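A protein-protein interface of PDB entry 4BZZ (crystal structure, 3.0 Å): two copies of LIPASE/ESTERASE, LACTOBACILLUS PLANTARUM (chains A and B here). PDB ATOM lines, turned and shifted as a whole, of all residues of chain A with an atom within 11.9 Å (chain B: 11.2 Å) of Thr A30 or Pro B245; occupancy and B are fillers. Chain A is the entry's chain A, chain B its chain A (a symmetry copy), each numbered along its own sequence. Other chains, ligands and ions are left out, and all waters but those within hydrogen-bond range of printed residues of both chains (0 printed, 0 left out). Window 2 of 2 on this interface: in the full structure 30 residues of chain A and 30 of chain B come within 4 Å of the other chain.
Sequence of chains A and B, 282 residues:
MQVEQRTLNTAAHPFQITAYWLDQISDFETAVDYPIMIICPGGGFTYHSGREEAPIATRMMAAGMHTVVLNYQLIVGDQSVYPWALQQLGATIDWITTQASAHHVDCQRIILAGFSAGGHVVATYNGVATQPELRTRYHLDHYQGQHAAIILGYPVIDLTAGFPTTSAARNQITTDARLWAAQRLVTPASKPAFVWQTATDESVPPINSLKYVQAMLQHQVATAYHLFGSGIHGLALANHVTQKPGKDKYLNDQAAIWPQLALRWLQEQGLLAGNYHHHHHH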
ATOM      1  N   ASP A  23       3.645  -6.284 -18.880  1.00  0.00           N
ATOM      2  CA  ASP A  23       3.984  -7.640 -18.450  1.00  0.00           C
ATOM      3  C   ASP A  23       3.850  -8.614 -19.614  1.00  0.00           C
ATOM      4  O   ASP A  23       3.087  -8.372 -20.551  1.00  0.00           O
ATOM      5  CB  ASP A  23       3.145  -8.073 -17.248  1.00  0.00           C
ATOM      6  CG  ASP A  23       3.770  -7.659 -15.920  1.00  0.00           C
ATOM      7  OD1 ASP A  23       4.995  -7.879 -15.748  1.00  0.00           O
ATOM      8  OD2 ASP A  23       3.041  -7.113 -15.053  1.00  0.00           O
ATOM      9  N   GLN A  24       4.630  -9.687 -19.574  1.00  0.00           N
ATOM     10  CA  GLN A  24       4.555 -10.703 -20.609  1.00  0.00           C
ATOM     11  C   GLN A  24       3.199 -11.394 -20.502  1.00  0.00           C
ATOM     12  O   GLN A  24       2.746 -11.736 -19.412  1.00  0.00           O
ATOM     13  CB  GLN A  24       5.673 -11.727 -20.436  1.00  0.00           C
ATOM     14  CG  GLN A  24       7.049 -11.224 -20.807  1.00  0.00           C
ATOM     15  CD  GLN A  24       7.121 -10.727 -22.236  1.00  0.00           C
ATOM     16  OE1 GLN A  24       7.126 -11.522 -23.178  1.00  0.00           O
ATOM     17  NE2 GLN A  24       7.179  -9.403 -22.406  1.00  0.00           N
ATOM     18  N   ILE A  25       2.543 -11.588 -21.635  1.00  0.00           N
ATOM     19  CA  ILE A  25       1.273 -12.293 -21.644  1.00  0.00           C
ATOM     20  C   ILE A  25       1.477 -13.760 -21.242  1.00  0.00           C
ATOM     21  O   ILE A  25       2.385 -14.431 -21.747  1.00  0.00           O
ATOM     22  CB  ILE A  25       0.598 -12.156 -23.009  1.00  0.00           C
ATOM     23  CG1 ILE A  25       0.043 -10.736 -23.148  1.00  0.00           C
ATOM     24  CG2 ILE A  25      -0.484 -13.216 -23.181  1.00  0.00           C
ATOM     25  CD1 ILE A  25      -0.274 -10.339 -24.537  1.00  0.00           C
ATOM     26  N   SER A  26       0.655 -14.248 -20.312  1.00  0.00           N
ATOM     27  CA  SER A  26       0.921 -15.545 -19.697  1.00  0.00           C
ATOM     28  C   SER A  26       0.826 -16.717 -20.674  1.00  0.00           C
ATOM     29  O   SER A  26       1.674 -17.606 -20.660  1.00  0.00           O
ATOM     30  CB  SER A  26       0.032 -15.770 -18.480  1.00  0.00           C
ATOM     31  OG  SER A  26      -1.331 -15.743 -18.847  1.00  0.00           O
ATOM     32  N   ASP A  27      -0.189 -16.715 -21.531  1.00  0.00           N
ATOM     33  CA  ASP A  27      -0.377 -17.835 -22.450  1.00  0.00           C
ATOM     34  C   ASP A  27       0.321 -17.667 -23.794  1.00  0.00           C
ATOM     35  O   ASP A  27      -0.205 -18.075 -24.823  1.00  0.00           O
ATOM     36  CB  ASP A  27      -1.864 -18.165 -22.652  1.00  0.00           C
ATOM     37  CG  ASP A  27      -2.752 -16.956 -22.564  1.00  0.00           C
ATOM     38  OD1 ASP A  27      -2.600 -16.186 -21.601  1.00  0.00           O
ATOM     39  OD2 ASP A  27      -3.615 -16.782 -23.445  1.00  0.00           O
ATOM     40  N   PHE A  28       1.501 -17.061 -23.785  1.00  0.00           N
ATOM     41  CA  PHE A  28       2.340 -17.051 -24.976  1.00  0.00           C
ATOM     42  C   PHE A  28       3.365 -18.144 -24.801  1.00  0.00           C
ATOM     43  O   PHE A  28       3.849 -18.371 -23.695  1.00  0.00           O
ATOM     44  CB  PHE A  28       3.067 -15.710 -25.166  1.00  0.00           C
ATOM     45  CG  PHE A  28       2.250 -14.656 -25.867  1.00  0.00           C
ATOM     46  CD1 PHE A  28       0.968 -14.927 -26.323  1.00  0.00           C
ATOM     47  CD2 PHE A  28       2.774 -13.385 -26.073  1.00  0.00           C
ATOM     48  CE1 PHE A  28       0.216 -13.941 -26.967  1.00  0.00           C
ATOM     49  CE2 PHE A  28       2.028 -12.399 -26.714  1.00  0.00           C
ATOM     50  CZ  PHE A  28       0.745 -12.678 -27.156  1.00  0.00           C
ATOM     51  N   GLU A  29       3.696 -18.821 -25.889  1.00  0.00           N
ATOM     52  CA  GLU A  29       4.777 -19.792 -25.865  1.00  0.00           C
ATOM     53  C   GLU A  29       6.138 -19.069 -25.864  1.00  0.00           C
ATOM     54  O   GLU A  29       7.009 -19.365 -25.051  1.00  0.00           O
ATOM     55  CB  GLU A  29       4.641 -20.765 -27.041  1.00  0.00           C
ATOM     56  CG  GLU A  29       3.258 -21.414 -27.129  1.00  0.00           C
ATOM     57  CD  GLU A  29       3.127 -22.412 -28.270  1.00  0.00           C
ATOM     58  OE1 GLU A  29       4.167 -22.937 -28.732  1.00  0.00           O
ATOM     59  OE2 GLU A  29       1.979 -22.667 -28.704  1.00  0.00           O
ATOM     60  N   THR A  30       6.315 -18.103 -26.758  1.00  0.00           N
ATOM     61  CA  THR A  30       7.569 -17.354 -26.788  1.00  0.00           C
ATOM     62  C   THR A  30       7.397 -15.910 -26.281  1.00  0.00           C
ATOM     63  O   THR A  30       6.317 -15.330 -26.391  1.00  0.00           O
ATOM     64  CB  THR A  30       8.261 -17.409 -28.189  1.00  0.00           C
ATOM     65  OG1 THR A  30       7.730 -16.396 -29.059  1.00  0.00           O
ATOM     66  CG2 THR A  30       8.100 -18.803 -28.820  1.00  0.00           C
ATOM     67  N   ALA A  31       8.454 -15.347 -25.702  1.00  0.00           N
ATOM     68  CA  ALA A  31       8.357 -14.018 -25.123  1.00  0.00           C
ATOM     69  C   ALA A  31       8.643 -12.970 -26.186  1.00  0.00           C
ATOM     70  O   ALA A  31       9.407 -13.213 -27.123  1.00  0.00           O
ATOM     71  CB  ALA A  31       9.314 -13.875 -23.960  1.00  0.00           C
ATOM     72  N   VAL A  32       8.027 -11.802 -26.050  1.00  0.00           N
ATOM     73  CA  VAL A  32       8.224 -10.755 -27.035  1.00  0.00           C
ATOM     74  C   VAL A  32       8.794  -9.483 -26.410  1.00  0.00           C
ATOM     75  O   VAL A  32       8.474  -9.144 -25.260  1.00  0.00           O
ATOM     76  CB  VAL A  32       6.929 -10.469 -27.839  1.00  0.00           C
ATOM     77  CG1 VAL A  32       5.864 -11.496 -27.516  1.00  0.00           C
ATOM     78  CG2 VAL A  32       6.421  -9.071 -27.586  1.00  0.00           C
ATOM     79  N   ASP A  33       9.665  -8.806 -27.163  1.00  0.00           N
ATOM     80  CA  ASP A  33      10.249  -7.555 -26.713  1.00  0.00           C
ATOM     81  C   ASP A  33       9.412  -6.414 -27.269  1.00  0.00           C
ATOM     82  O   ASP A  33       9.188  -6.323 -28.473  1.00  0.00           O
ATOM     83  CB  ASP A  33      11.710  -7.412 -27.169  1.00  0.00           C
ATOM     84  CG  ASP A  33      12.603  -8.531 -26.659  1.00  0.00           C
ATOM     85  OD1 ASP A  33      12.426  -8.950 -25.499  1.00  0.00           O
ATOM     86  OD2 ASP A  33      13.492  -8.988 -27.417  1.00  0.00           O
ATOM     87  N   TYR A  34       8.957  -5.540 -26.383  1.00  0.00           N
ATOM     88  CA  TYR A  34       8.066  -4.461 -26.765  1.00  0.00           C
ATOM     89  C   TYR A  34       8.835  -3.173 -26.953  1.00  0.00           C
ATOM     90  O   TYR A  34       9.906  -3.015 -26.377  1.00  0.00           O
ATOM     91  CB  TYR A  34       7.007  -4.278 -25.684  1.00  0.00           C
ATOM     92  CG  TYR A  34       6.076  -5.457 -25.566  1.00  0.00           C
ATOM     93  CD1 TYR A  34       5.036  -5.630 -26.460  1.00  0.00           C
ATOM     94  CD2 TYR A  34       6.243  -6.399 -24.568  1.00  0.00           C
ATOM     95  CE1 TYR A  34       4.187  -6.710 -26.360  1.00  0.00           C
ATOM     96  CE2 TYR A  34       5.398  -7.478 -24.459  1.00  0.00           C
ATOM     97  CZ  TYR A  34       4.368  -7.629 -25.356  1.00  0.00           C
ATOM     98  OH  TYR A  34       3.522  -8.704 -25.262  1.00  0.00           O
ATOM     99  N   HIS A 103      12.654  -6.466 -18.439  1.00  0.00           N
ATOM    100  CA  HIS A 103      11.328  -6.030 -18.868  1.00  0.00           C
ATOM    101  C   HIS A 103      10.991  -6.285 -20.337  1.00  0.00           C
ATOM    102  O   HIS A 103       9.954  -5.823 -20.822  1.00  0.00           O
ATOM    103  CB  HIS A 103      11.144  -4.543 -18.572  1.00  0.00           C
ATOM    104  CG  HIS A 103      11.115  -4.210 -17.116  1.00  0.00           C
ATOM    105  ND1 HIS A 103       9.965  -4.286 -16.357  1.00  0.00           N
ATOM    106  CD2 HIS A 103      12.092  -3.785 -16.279  1.00  0.00           C
ATOM    107  CE1 HIS A 103      10.237  -3.925 -15.115  1.00  0.00           C
ATOM    108  NE2 HIS A 103      11.521  -3.612 -15.043  1.00  0.00           N
ATOM    109  N   HIS A 104      11.849  -7.011 -21.042  1.00  0.00           N
ATOM    110  CA  HIS A 104      11.648  -7.247 -22.477  1.00  0.00           C
ATOM    111  C   HIS A 104      11.453  -5.938 -23.251  1.00  0.00           C
ATOM    112  O   HIS A 104      10.339  -5.596 -23.645  1.00  0.00           O
ATOM    113  CB  HIS A 104      10.484  -8.222 -22.741  1.00  0.00           C
ATOM    114  CG  HIS A 104      10.701  -9.589 -22.169  1.00  0.00           C
ATOM    115  ND1 HIS A 104      10.238  -9.960 -20.923  1.00  0.00           N
ATOM    116  CD2 HIS A 104      11.351 -10.670 -22.665  1.00  0.00           C
ATOM    117  CE1 HIS A 104      10.590 -11.210 -20.678  1.00  0.00           C
ATOM    118  NE2 HIS A 104      11.268 -11.663 -21.718  1.00  0.00           N
ATOM    119  N   ALA A 273       4.922  -3.320 -34.218  1.00  0.00           N
ATOM    120  CA  ALA A 273       4.398  -4.447 -34.985  1.00  0.00           C
ATOM    121  C   ALA A 273       3.081  -4.072 -35.685  1.00  0.00           C
ATOM    122  O   ALA A 273       2.274  -3.314 -35.140  1.00  0.00           O
ATOM    123  CB  ALA A 273       4.207  -5.624 -34.080  1.00  0.00           C
ATOM    124  N   GLY A 274       2.876  -4.589 -36.895  1.00  0.00           N
ATOM    125  CA  GLY A 274       1.723  -4.219 -37.706  1.00  0.00           C
ATOM    126  C   GLY A 274       0.665  -5.303 -37.815  1.00  0.00           C
ATOM    127  O   GLY A 274       0.972  -6.495 -37.726  1.00  0.00           O
ATOM    128  N   ARG B  51      -4.169 -12.949 -22.400  1.00  0.00           N
ATOM    129  CA  ARG B  51      -4.568 -12.223 -23.598  1.00  0.00           C
ATOM    130  C   ARG B  51      -5.806 -11.373 -23.402  1.00  0.00           C
ATOM    131  O   ARG B  51      -5.923 -10.324 -24.013  1.00  0.00           O
ATOM    132  CB  ARG B  51      -4.799 -13.202 -24.751  1.00  0.00           C
ATOM    133  CG  ARG B  51      -3.571 -14.031 -25.049  1.00  0.00           C
ATOM    134  CD  ARG B  51      -3.715 -14.837 -26.322  1.00  0.00           C
ATOM    135  NE  ARG B  51      -4.190 -14.020 -27.427  1.00  0.00           N
ATOM    136  CZ  ARG B  51      -5.378 -14.172 -27.995  1.00  0.00           C
ATOM    137  NH1 ARG B  51      -6.196 -15.125 -27.564  1.00  0.00           N
ATOM    138  NH2 ARG B  51      -5.738 -13.380 -28.995  1.00  0.00           N
ATOM    139  N   ILE B 232     -11.044 -16.329 -36.110  1.00  0.00           N
ATOM    140  CA  ILE B 232     -11.163 -17.438 -35.168  1.00  0.00           C
ATOM    141  C   ILE B 232     -11.733 -17.007 -33.809  1.00  0.00           C
ATOM    142  O   ILE B 232     -12.033 -15.831 -33.581  1.00  0.00           O
ATOM    143  CB  ILE B 232      -9.812 -18.157 -34.942  1.00  0.00           C
ATOM    144  CG1 ILE B 232      -8.808 -17.217 -34.273  1.00  0.00           C
ATOM    145  CG2 ILE B 232      -9.274 -18.701 -36.249  1.00  0.00           C
ATOM    146  CD1 ILE B 232      -7.538 -17.913 -33.836  1.00  0.00           C
ATOM    147  N   GLY B 234     -11.436 -16.236 -29.856  1.00  0.00           N
ATOM    148  CA  GLY B 234     -10.426 -15.706 -28.955  1.00  0.00           C
ATOM    149  C   GLY B 234      -9.481 -14.737 -29.629  1.00  0.00           C
ATOM    150  O   GLY B 234      -8.268 -14.791 -29.418  1.00  0.00           O
ATOM    151  N   ASN B 239      -5.538  -7.499 -32.795  1.00  0.00           N
ATOM    152  CA  ASN B 239      -4.364  -6.854 -33.363  1.00  0.00           C
ATOM    153  C   ASN B 239      -3.041  -7.399 -32.829  1.00  0.00           C
ATOM    154  O   ASN B 239      -3.014  -8.422 -32.160  1.00  0.00           O
ATOM    155  CB  ASN B 239      -4.458  -5.342 -33.191  1.00  0.00           C
ATOM    156  CG  ASN B 239      -4.420  -4.915 -31.754  1.00  0.00           C
ATOM    157  OD1 ASN B 239      -4.148  -5.711 -30.865  1.00  0.00           O
ATOM    158  ND2 ASN B 239      -4.683  -3.639 -31.515  1.00  0.00           N
ATOM    159  N   HIS B 240      -1.950  -6.702 -33.119  1.00  0.00           N
ATOM    160  CA  HIS B 240      -0.601  -7.165 -32.776  1.00  0.00           C
ATOM    161  C   HIS B 240      -0.365  -7.358 -31.282  1.00  0.00           C
ATOM    162  O   HIS B 240       0.501  -8.125 -30.879  1.00  0.00           O
ATOM    163  CB  HIS B 240       0.462  -6.211 -33.348  1.00  0.00           C
ATOM    164  CG  HIS B 240       0.507  -4.867 -32.680  1.00  0.00           C
ATOM    165  ND1 HIS B 240      -0.434  -3.885 -32.912  1.00  0.00           N
ATOM    166  CD2 HIS B 240       1.393  -4.337 -31.803  1.00  0.00           C
ATOM    167  CE1 HIS B 240      -0.138  -2.813 -32.197  1.00  0.00           C
ATOM    168  NE2 HIS B 240       0.966  -3.062 -31.516  1.00  0.00           N
ATOM    169  N   VAL B 241      -1.137  -6.663 -30.464  1.00  0.00           N
ATOM    170  CA  VAL B 241      -0.930  -6.683 -29.029  1.00  0.00           C
ATOM    171  C   VAL B 241      -1.261  -8.053 -28.429  1.00  0.00           C
ATOM    172  O   VAL B 241      -0.487  -8.585 -27.633  1.00  0.00           O
ATOM    173  CB  VAL B 241      -1.718  -5.550 -28.350  1.00  0.00           C
ATOM    174  CG1 VAL B 241      -1.345  -5.438 -26.903  1.00  0.00           C
ATOM    175  CG2 VAL B 241      -1.428  -4.252 -29.058  1.00  0.00           C
ATOM    176  N   THR B 242      -2.388  -8.629 -28.838  1.00  0.00           N
ATOM    177  CA  THR B 242      -2.809  -9.956 -28.370  1.00  0.00           C
ATOM    178  C   THR B 242      -2.547 -11.081 -29.383  1.00  0.00           C
ATOM    179  O   THR B 242      -3.089 -12.179 -29.252  1.00  0.00           O
ATOM    180  CB  THR B 242      -4.307  -9.985 -28.041  1.00  0.00           C
ATOM    181  OG1 THR B 242      -5.072  -9.716 -29.229  1.00  0.00           O
ATOM    182  CG2 THR B 242      -4.628  -8.972 -26.974  1.00  0.00           C
ATOM    183  N   GLN B 243      -1.732 -10.807 -30.396  1.00  0.00           N
ATOM    184  CA  GLN B 243      -1.433 -11.813 -31.404  1.00  0.00           C
ATOM    185  C   GLN B 243      -0.354 -12.759 -30.901  1.00  0.00           C
ATOM    186  O   GLN B 243       0.753 -12.309 -30.592  1.00  0.00           O
ATOM    187  CB  GLN B 243      -0.951 -11.156 -32.706  1.00  0.00           C
ATOM    188  CG  GLN B 243      -0.725 -12.157 -33.837  1.00  0.00           C
ATOM    189  CD  GLN B 243       0.325 -11.710 -34.834  1.00  0.00           C
ATOM    190  OE1 GLN B 243       0.725 -10.550 -34.851  1.00  0.00           O
ATOM    191  NE2 GLN B 243       0.782 -12.639 -35.669  1.00  0.00           N
ATOM    192  N   LYS B 244      -0.660 -14.057 -30.819  1.00  0.00           N
ATOM    193  CA  LYS B 244       0.369 -15.052 -30.507  1.00  0.00           C
ATOM    194  C   LYS B 244       1.453 -14.999 -31.575  1.00  0.00           C
ATOM    195  O   LYS B 244       1.145 -15.036 -32.764  1.00  0.00           O
ATOM    196  CB  LYS B 244      -0.221 -16.458 -30.427  1.00  0.00           C
ATOM    197  CG  LYS B 244      -1.145 -16.669 -29.242  1.00  0.00           C
ATOM    198  CD  LYS B 244      -1.542 -18.131 -29.105  1.00  0.00           C
ATOM    199  CE  LYS B 244      -2.464 -18.352 -27.913  1.00  0.00           C
ATOM    200  NZ  LYS B 244      -2.820 -19.790 -27.726  1.00  0.00           N
ATOM    201  N   PRO B 245       2.726 -14.895 -31.154  1.00  0.00           N
ATOM    202  CA  PRO B 245       3.889 -14.722 -32.047  1.00  0.00           C
ATOM    203  C   PRO B 245       3.928 -15.705 -33.227  1.00  0.00           C
ATOM    204  O   PRO B 245       3.965 -16.929 -33.029  1.00  0.00           O
ATOM    205  CB  PRO B 245       5.081 -14.963 -31.118  1.00  0.00           C
ATOM    206  CG  PRO B 245       4.587 -14.533 -29.783  1.00  0.00           C
ATOM    207  CD  PRO B 245       3.124 -14.918 -29.735  1.00  0.00           C
ATOM    208  N   GLY B 246       3.909 -15.158 -34.440  1.00  0.00           N
ATOM    209  CA  GLY B 246       3.986 -15.964 -35.644  1.00  0.00           C
ATOM    210  C   GLY B 246       2.645 -16.275 -36.279  1.00  0.00           C
ATOM    211  O   GLY B 246       2.560 -16.388 -37.502  1.00  0.00           O
ATOM    212  N   LYS B 247       1.604 -16.404 -35.455  1.00  0.00           N
ATOM    213  CA  LYS B 247       0.301 -16.898 -35.915  1.00  0.00           C
ATOM    214  C   LYS B 247      -0.655 -15.792 -36.370  1.00  0.00           C
ATOM    215  O   LYS B 247      -1.247 -15.094 -35.549  1.00  0.00           O
ATOM    216  CB  LYS B 247      -0.363 -17.787 -34.846  1.00  0.00           C
ATOM    217  CG  LYS B 247       0.347 -19.128 -34.605  1.00  0.00           C
ATOM    218  CD  LYS B 247      -0.540 -20.123 -33.858  1.00  0.00           C
ATOM    219  CE  LYS B 247       0.159 -21.467 -33.637  1.00  0.00           C
ATOM    220  NZ  LYS B 247       1.206 -21.410 -32.571  1.00  0.00           N
ATOM    221  N   ASP B 248      -0.817 -15.665 -37.685  1.00  0.00           N
ATOM    222  CA  ASP B 248      -1.601 -14.588 -38.286  1.00  0.00           C
ATOM    223  C   ASP B 248      -3.101 -14.771 -38.097  1.00  0.00           C
ATOM    224  O   ASP B 248      -3.883 -13.864 -38.391  1.00  0.00           O
ATOM    225  CB  ASP B 248      -1.280 -14.476 -39.778  1.00  0.00           C
ATOM    226  CG  ASP B 248       0.201 -14.296 -40.039  1.00  0.00           C
ATOM    227  OD1 ASP B 248       0.807 -13.411 -39.398  1.00  0.00           O
ATOM    228  OD2 ASP B 248       0.761 -15.042 -40.877  1.00  0.00           O
ATOM    229  N   LYS B 249      -3.498 -15.944 -37.607  1.00  0.00           N
ATOM    230  CA  LYS B 249      -4.917 -16.258 -37.418  1.00  0.00           C
ATOM    231  C   LYS B 249      -5.538 -15.469 -36.257  1.00  0.00           C
ATOM    232  O   LYS B 249      -6.763 -15.446 -36.097  1.00  0.00           O
ATOM    233  CB  LYS B 249      -5.146 -17.774 -37.273  1.00  0.00           C
ATOM    234  CG  LYS B 249      -4.424 -18.428 -36.104  1.00  0.00           C
ATOM    235  CD  LYS B 249      -4.669 -19.932 -36.069  1.00  0.00           C
ATOM    236  CE  LYS B 249      -3.981 -20.590 -34.870  1.00  0.00           C
ATOM    237  NZ  LYS B 249      -4.109 -22.083 -34.834  1.00  0.00           N
ATOM    238  N   TYR B 250      -4.687 -14.803 -35.474  1.00  0.00           N
ATOM    239  CA  TYR B 250      -5.135 -13.924 -34.393  1.00  0.00           C
ATOM    240  C   TYR B 250      -5.213 -12.459 -34.813  1.00  0.00           C
ATOM    241  O   TYR B 250      -5.371 -11.575 -33.967  1.00  0.00           O
ATOM    242  CB  TYR B 250      -4.226 -14.071 -33.173  1.00  0.00           C
ATOM    243  CG  TYR B 250      -4.439 -15.370 -32.445  1.00  0.00           C
ATOM    244  CD1 TYR B 250      -5.463 -15.500 -31.518  1.00  0.00           C
ATOM    245  CD2 TYR B 250      -3.635 -16.474 -32.700  1.00  0.00           C
ATOM    246  CE1 TYR B 250      -5.676 -16.685 -30.857  1.00  0.00           C
ATOM    247  CE2 TYR B 250      -3.839 -17.664 -32.039  1.00  0.00           C
ATOM    248  CZ  TYR B 250      -4.864 -17.764 -31.116  1.00  0.00           C
ATOM    249  OH  TYR B 250      -5.090 -18.946 -30.444  1.00  0.00           O
ATOM    250  N   LEU B 251      -5.096 -12.206 -36.115  1.00  0.00           N
ATOM    251  CA  LEU B 251      -5.243 -10.852 -36.649  1.00  0.00           C
ATOM    252  C   LEU B 251      -6.508 -10.714 -37.489  1.00  0.00           C
ATOM    253  O   LEU B 251      -6.680 -11.419 -38.483  1.00  0.00           O
ATOM    254  CB  LEU B 251      -4.038 -10.466 -37.508  1.00  0.00           C
ATOM    255  CG  LEU B 251      -2.702 -10.364 -36.792  1.00  0.00           C
ATOM    256  CD1 LEU B 251      -1.639  -9.879 -37.734  1.00  0.00           C
ATOM    257  CD2 LEU B 251      -2.853  -9.438 -35.598  1.00  0.00           C
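OD1 of Asn B239 lies close to N of Val B241 (3.2 Å). The guanidinium group (NH1) of Arg B51 is in hydrogen-bond range of the backbone carbonyl oxygen (O) of Gly B234. The side-chain amide nitrogen of Gln B243 sits at hydrogen-bond distance from the backbone carbonyl oxygen of Lys B247 (3.2 Å). The backbone NH of Val A32 lies within hydrogen-bond range of the side-chain amide oxygen of Gln A24, at 3.0 Å. The guanidinium group (NE) of Arg B51 sits at hydrogen-bond distance from the backbone carbonyl oxygen (O) of Thr B242. OG of Ser A26 is in hydrogen-bond range of OD1 of Asp A27, 3.1 Å away.
Among the printed residues, pairs that only touch across the chains: Ile A25 with Arg B51, Ile A25 with Val B241, Asp A27 with Arg B51, Asp A27 with Lys B244, Phe A28 with Gln B243, Phe A28 with Lys B244, Phe A28 with Pro B245, Thr A30 with Pro B245, Val A32 with Pro B245 and Ala A273 with His B240.
Thr A30 touches just one residue of chain B: Pro B245 (3.6 Å). Of the printed residues of chain A, Pro B245 touches Phe A28 (3.97 Å), Thr A30 (3.6 Å) and Val A32 (3.999 Å). Of the printed residues of chain B, Phe A28 touches Gln B243 (3.5 Å), Lys B244 (3.7 Å) and Pro B245 (3.97 Å). No residue of chain B comes within 4 Å of Glu A29. No residue of chain B comes within 4 Å of Ala A31. Printed residues of chain A within 4 Å of Gln B243: Phe A28. No residue of chain A comes within 4 Å of Gly B246. No residue of chain A comes within 4 Å of Lys B247. Of the printed residues of chain A, Arg B51 touches Ile A25 (3.7 Å) and Asp A27 (3.2 Å). Printed residues of chain B within 4 Å of Ala A273: His B240 (3.4 Å). Of the printed residues of chain A, Lys B244 touches Asp A27 (3.8 Å) and Phe A28 (3.7 Å). His A103 touches none of the printed residues of chain B. The nearest residue of chain B that does not touch Thr A30 is Gly B246 (6.7 Å).
Hydrophobic or aromatic side chains of chain A within 4 Å of the printed part of chain B: Ile A25, Phe A28, Val A32 and Ala A273. Printed residues of chain B that touch a printed residue of chain A: Arg B51, His B240, Val B241, Gln B243, Lys B244 and Pro B245. Hydrophobic or aromatic side chains of chain B within 4 Å of the printed part of chain A: His B240 and Pro B245.
No position is printed for both chains. Of the 10 pairs that touch across the chains among the printed residues, none has its exchanged pair printed and touching as well.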
